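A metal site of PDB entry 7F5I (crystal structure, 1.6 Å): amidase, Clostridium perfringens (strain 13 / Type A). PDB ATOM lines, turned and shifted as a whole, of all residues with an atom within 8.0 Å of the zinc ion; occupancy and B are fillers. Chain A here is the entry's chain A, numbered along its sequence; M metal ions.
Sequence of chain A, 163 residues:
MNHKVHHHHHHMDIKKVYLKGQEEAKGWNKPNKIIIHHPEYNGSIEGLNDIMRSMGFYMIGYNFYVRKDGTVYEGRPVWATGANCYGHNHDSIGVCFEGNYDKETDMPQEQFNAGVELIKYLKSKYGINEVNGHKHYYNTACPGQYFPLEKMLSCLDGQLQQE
Within 4 Å of the zinc ion: His 37, His 134 and Cys 142.
O of Ile 36 is in hydrogen-bond range of N of His 134, 2.9 Å away. SG of Cys 85 sits close to NE2 of His 134. A ring nitrogen (NE2) of His 37 sits at hydrogen-bond distance from the side-chain amide oxygen (OD1) of Asn 84 (2.8 Å). N of His 37 lies within hydrogen-bond range of O of Val 95, at 2.9 Å. The backbone NH (N) of His 38 sits close to the side-chain sulfur (SG) of Cys 142, 3.5 Å away. The side-chain hydroxyl (OG1) of Thr 140 sits at hydrogen-bond distance from the backbone NH (N) of Cys 142, 3.0 Å away. The backbone carbonyl oxygen (O) of Cys 142 lies within hydrogen-bond range of the backbone NH (N) of Lys 135 (2.9 Å).
The zinc ion is bound by a ring nitrogen (ND1) of His 134, a ring nitrogen (ND1) of His 37 and the side-chain sulfur of Cys 142. The zinc ion has three donor atoms within binding distance.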
ATOM      1  N   ILE A  35     -20.942  14.351  17.476  1.00  0.00           N
ATOM      2  CA  ILE A  35     -20.307  15.695  17.385  1.00  0.00           C
ATOM      3  C   ILE A  35     -19.867  16.086  18.790  1.00  0.00           C
ATOM      4  O   ILE A  35     -20.715  16.035  19.729  1.00  0.00           O
ATOM      5  CB  ILE A  35     -21.217  16.721  16.707  1.00  0.00           C
ATOM      6  CG1 ILE A  35     -21.742  16.192  15.354  1.00  0.00           C
ATOM      7  CG2 ILE A  35     -20.454  18.021  16.535  1.00  0.00           C
ATOM      8  CD1 ILE A  35     -22.651  17.154  14.611  1.00  0.00           C
ATOM      9  N   ILE A  36     -18.569  16.389  18.924  1.00  0.00           N
ATOM     10  CA  ILE A  36     -17.923  16.723  20.218  1.00  0.00           C
ATOM     11  C   ILE A  36     -17.925  18.242  20.382  1.00  0.00           C
ATOM     12  O   ILE A  36     -17.520  18.997  19.472  1.00  0.00           O
ATOM     13  CB  ILE A  36     -16.503  16.116  20.254  1.00  0.00           C
ATOM     14  CG1 ILE A  36     -16.576  14.584  20.242  1.00  0.00           C
ATOM     15  CG2 ILE A  36     -15.767  16.640  21.464  1.00  0.00           C
ATOM     16  CD1 ILE A  36     -15.248  13.894  20.070  1.00  0.00           C
ATOM     17  N   HIS A  37     -18.315  18.681  21.573  1.00  0.00           N
ATOM     18  CA  HIS A  37     -18.462  20.101  21.914  1.00  0.00           C
ATOM     19  C   HIS A  37     -17.836  20.372  23.271  1.00  0.00           C
ATOM     20  O   HIS A  37     -17.751  19.438  24.071  1.00  0.00           O
ATOM     21  CB  HIS A  37     -19.947  20.512  22.002  1.00  0.00           C
ATOM     22  CG  HIS A  37     -20.739  20.276  20.763  1.00  0.00           C
ATOM     23  ND1 HIS A  37     -20.862  21.237  19.772  1.00  0.00           N
ATOM     24  CD2 HIS A  37     -21.536  19.229  20.404  1.00  0.00           C
ATOM     25  CE1 HIS A  37     -21.691  20.786  18.852  1.00  0.00           C
ATOM     26  NE2 HIS A  37     -22.101  19.553  19.202  1.00  0.00           N
ATOM     27  N   HIS A  38     -17.528  21.634  23.512  1.00  0.00           N
ATOM     28  CA  HIS A  38     -17.479  22.231  24.871  1.00  0.00           C
ATOM     29  C   HIS A  38     -18.508  23.353  24.914  1.00  0.00           C
ATOM     30  O   HIS A  38     -19.008  23.828  23.891  1.00  0.00           O
ATOM     31  CB  HIS A  38     -16.050  22.672  25.234  1.00  0.00           C
ATOM     32  CG  HIS A  38     -15.612  23.922  24.558  1.00  0.00           C
ATOM     33  ND1 HIS A  38     -14.628  24.721  25.082  1.00  0.00           N
ATOM     34  CD2 HIS A  38     -16.004  24.515  23.399  1.00  0.00           C
ATOM     35  CE1 HIS A  38     -14.414  25.754  24.285  1.00  0.00           C
ATOM     36  NE2 HIS A  38     -15.255  25.657  23.238  1.00  0.00           N
ATOM     37  N   PRO A  39     -18.959  23.744  26.113  1.00  0.00           N
ATOM     38  CA  PRO A  39     -19.892  24.863  26.235  1.00  0.00           C
ATOM     39  C   PRO A  39     -19.304  26.203  26.701  1.00  0.00           C
ATOM     40  O   PRO A  39     -20.073  27.169  26.824  1.00  0.00           O
ATOM     41  CB  PRO A  39     -20.806  24.261  27.298  1.00  0.00           C
ATOM     42  CG  PRO A  39     -19.876  23.554  28.266  1.00  0.00           C
ATOM     43  CD  PRO A  39     -18.743  23.044  27.389  1.00  0.00           C
ATOM     44  N   TYR A  62     -27.544  19.814  23.732  1.00  0.00           N
ATOM     45  CA  TYR A  62     -26.699  18.603  23.703  1.00  0.00           C
ATOM     46  C   TYR A  62     -27.492  17.373  24.192  1.00  0.00           C
ATOM     47  O   TYR A  62     -28.345  17.518  25.093  1.00  0.00           O
ATOM     48  CB  TYR A  62     -25.486  18.812  24.601  1.00  0.00           C
ATOM     49  CG  TYR A  62     -24.697  20.070  24.336  1.00  0.00           C
ATOM     50  CD1 TYR A  62     -23.938  20.229  23.184  1.00  0.00           C
ATOM     51  CD2 TYR A  62     -24.653  21.085  25.276  1.00  0.00           C
ATOM     52  CE1 TYR A  62     -23.181  21.364  22.949  1.00  0.00           C
ATOM     53  CE2 TYR A  62     -23.897  22.217  25.070  1.00  0.00           C
ATOM     54  CZ  TYR A  62     -23.156  22.363  23.909  1.00  0.00           C
ATOM     55  OH  TYR A  62     -22.380  23.466  23.779  1.00  0.00           O
ATOM     56  N   ASN A  84     -27.680  20.770  18.540  1.00  0.00           N
ATOM     57  CA  ASN A  84     -26.224  20.815  18.880  1.00  0.00           C
ATOM     58  C   ASN A  84     -25.392  21.406  17.727  1.00  0.00           C
ATOM     59  O   ASN A  84     -24.319  21.964  17.997  1.00  0.00           O
ATOM     60  CB  ASN A  84     -25.728  19.448  19.352  1.00  0.00           C
ATOM     61  CG  ASN A  84     -25.372  18.490  18.240  1.00  0.00           C
ATOM     62  OD1 ASN A  84     -24.212  18.447  17.816  1.00  0.00           O
ATOM     63  ND2 ASN A  84     -26.355  17.689  17.817  1.00  0.00           N
ATOM     64  N   CYS A  85     -25.844  21.291  16.472  1.00  0.00           N
ATOM     65  CA  CYS A  85     -25.066  21.723  15.291  1.00  0.00           C
ATOM     66  C   CYS A  85     -25.990  22.080  14.125  1.00  0.00           C
ATOM     67  O   CYS A  85     -26.726  21.198  13.668  1.00  0.00           O
ATOM     68  CB  CYS A  85     -24.059  20.648  14.919  1.00  0.00           C
ATOM     69  SG  CYS A  85     -22.925  21.183  13.604  1.00  0.00           S
ATOM     70  N   VAL A  95     -22.321  15.477  21.967  1.00  0.00           N
ATOM     71  CA  VAL A  95     -21.699  15.184  23.273  1.00  0.00           C
ATOM     72  C   VAL A  95     -20.932  16.428  23.736  1.00  0.00           C
ATOM     73  O   VAL A  95     -20.028  16.893  23.042  1.00  0.00           O
ATOM     74  CB  VAL A  95     -20.801  13.948  23.188  1.00  0.00           C
ATOM     75  CG1 VAL A  95     -20.128  13.707  24.535  1.00  0.00           C
ATOM     76  CG2 VAL A  95     -21.582  12.732  22.736  1.00  0.00           C
ATOM     77  N   CYS A  96     -21.319  16.964  24.883  1.00  0.00           N
ATOM     78  CA  CYS A  96     -20.681  18.149  25.464  1.00  0.00           C
ATOM     79  C   CYS A  96     -19.787  17.734  26.643  1.00  0.00           C
ATOM     80  O   CYS A  96     -20.238  16.968  27.532  1.00  0.00           O
ATOM     81  CB  CYS A  96     -21.741  19.157  25.877  1.00  0.00           C
ATOM     82  SG  CYS A  96     -21.058  20.680  26.560  1.00  0.00           S
ATOM     83  N   GLY A 133     -15.071  16.783  16.020  1.00  0.00           N
ATOM     84  CA  GLY A 133     -15.325  18.058  16.703  1.00  0.00           C
ATOM     85  C   GLY A 133     -16.356  18.854  15.939  1.00  0.00           C
ATOM     86  O   GLY A 133     -16.383  18.770  14.712  1.00  0.00           O
ATOM     87  N   HIS A 134     -17.146  19.655  16.663  1.00  0.00           N
ATOM     88  CA  HIS A 134     -18.069  20.639  16.061  1.00  0.00           C
ATOM     89  C   HIS A 134     -17.403  21.351  14.880  1.00  0.00           C
ATOM     90  O   HIS A 134     -18.075  21.520  13.835  1.00  0.00           O
ATOM     91  CB  HIS A 134     -18.559  21.595  17.156  1.00  0.00           C
ATOM     92  CG  HIS A 134     -19.696  22.490  16.795  1.00  0.00           C
ATOM     93  ND1 HIS A 134     -20.323  23.281  17.724  1.00  0.00           N
ATOM     94  CD2 HIS A 134     -20.362  22.656  15.629  1.00  0.00           C
ATOM     95  CE1 HIS A 134     -21.306  23.945  17.138  1.00  0.00           C
ATOM     96  NE2 HIS A 134     -21.354  23.576  15.839  1.00  0.00           N
ATOM     97  N   LYS A 135     -16.140  21.780  15.042  1.00  0.00           N
ATOM     98  CA  LYS A 135     -15.382  22.585  14.046  1.00  0.00           C
ATOM     99  C   LYS A 135     -15.267  21.839  12.713  1.00  0.00           C
ATOM    100  O   LYS A 135     -15.020  22.495  11.697  1.00  0.00           O
ATOM    101  CB  LYS A 135     -13.959  22.901  14.535  1.00  0.00           C
ATOM    102  CG  LYS A 135     -13.097  21.678  14.828  1.00  0.00           C
ATOM    103  CD  LYS A 135     -11.704  21.980  15.387  1.00  0.00           C
ATOM    104  CE  LYS A 135     -11.713  22.953  16.554  1.00  0.00           C
ATOM    105  NZ  LYS A 135     -10.444  22.917  17.331  1.00  0.00           N
ATOM    106  N   TYR A 138     -18.918  22.956  11.075  1.00  0.00           N
ATOM    107  CA  TYR A 138     -19.458  24.333  11.231  1.00  0.00           C
ATOM    108  C   TYR A 138     -18.277  25.250  11.509  1.00  0.00           C
ATOM    109  O   TYR A 138     -17.286  24.765  12.075  1.00  0.00           O
ATOM    110  CB  TYR A 138     -20.511  24.370  12.338  1.00  0.00           C
ATOM    111  CG  TYR A 138     -21.217  25.698  12.520  1.00  0.00           C
ATOM    112  CD1 TYR A 138     -22.270  26.089  11.696  1.00  0.00           C
ATOM    113  CD2 TYR A 138     -20.825  26.571  13.516  1.00  0.00           C
ATOM    114  CE1 TYR A 138     -22.920  27.308  11.884  1.00  0.00           C
ATOM    115  CE2 TYR A 138     -21.465  27.790  13.709  1.00  0.00           C
ATOM    116  CZ  TYR A 138     -22.513  28.159  12.892  1.00  0.00           C
ATOM    117  OH  TYR A 138     -23.098  29.374  13.108  1.00  0.00           O
ATOM    118  N   THR A 140     -16.661  27.195  13.592  1.00  0.00           N
ATOM    119  CA  THR A 140     -16.481  27.438  15.051  1.00  0.00           C
ATOM    120  C   THR A 140     -15.126  26.872  15.487  1.00  0.00           C
ATOM    121  O   THR A 140     -14.611  25.960  14.807  1.00  0.00           O
ATOM    122  CB  THR A 140     -17.612  26.830  15.876  1.00  0.00           C
ATOM    123  OG1 THR A 140     -17.386  27.101  17.258  1.00  0.00           O
ATOM    124  CG2 THR A 140     -17.761  25.329  15.712  1.00  0.00           C
ATOM    125  N   ALA A 141     -14.580  27.405  16.580  1.00  0.00           N
ATOM    126  CA  ALA A 141     -13.396  26.867  17.277  1.00  0.00           C
ATOM    127  C   ALA A 141     -13.817  25.689  18.158  1.00  0.00           C
ATOM    128  O   ALA A 141     -12.928  24.913  18.533  1.00  0.00           O
ATOM    129  CB  ALA A 141     -12.717  27.968  18.060  1.00  0.00           C
ATOM    130  N   CYS A 142     -15.104  25.548  18.466  1.00  0.00           N
ATOM    131  CA  CYS A 142     -15.630  24.445  19.325  1.00  0.00           C
ATOM    132  C   CYS A 142     -15.142  23.111  18.750  1.00  0.00           C
ATOM    133  O   CYS A 142     -15.273  22.913  17.546  1.00  0.00           O
ATOM    134  CB  CYS A 142     -17.150  24.473  19.411  1.00  0.00           C
ATOM    135  SG  CYS A 142     -17.875  23.161  20.430  1.00  0.00           S
ATOM    136  N   PRO A 143     -14.578  22.160  19.543  1.00  0.00           N
ATOM    137  CA  PRO A 143     -14.547  22.164  21.011  1.00  0.00           C
ATOM    138  C   PRO A 143     -13.339  22.803  21.729  1.00  0.00           C
ATOM    139  O   PRO A 143     -13.141  22.505  22.903  1.00  0.00           O
ATOM    140  CB  PRO A 143     -14.543  20.653  21.341  1.00  0.00           C
ATOM    141  CG  PRO A 143     -13.688  20.073  20.233  1.00  0.00           C
ATOM    142  CD  PRO A 143     -14.117  20.871  19.015  1.00  0.00           C
ATOM    143  N   GLY A 144     -12.587  23.676  21.046  1.00  0.00           N
ATOM    144  CA  GLY A 144     -11.581  24.565  21.663  1.00  0.00           C
ATOM    145  C   GLY A 144     -10.171  24.130  21.332  1.00  0.00           C
ATOM    146  O   GLY A 144      -9.928  22.905  21.157  1.00  0.00           O
HETATM  147 ZN    ZN M   1     -20.028  23.100  19.703  1.00  0.00          ZN
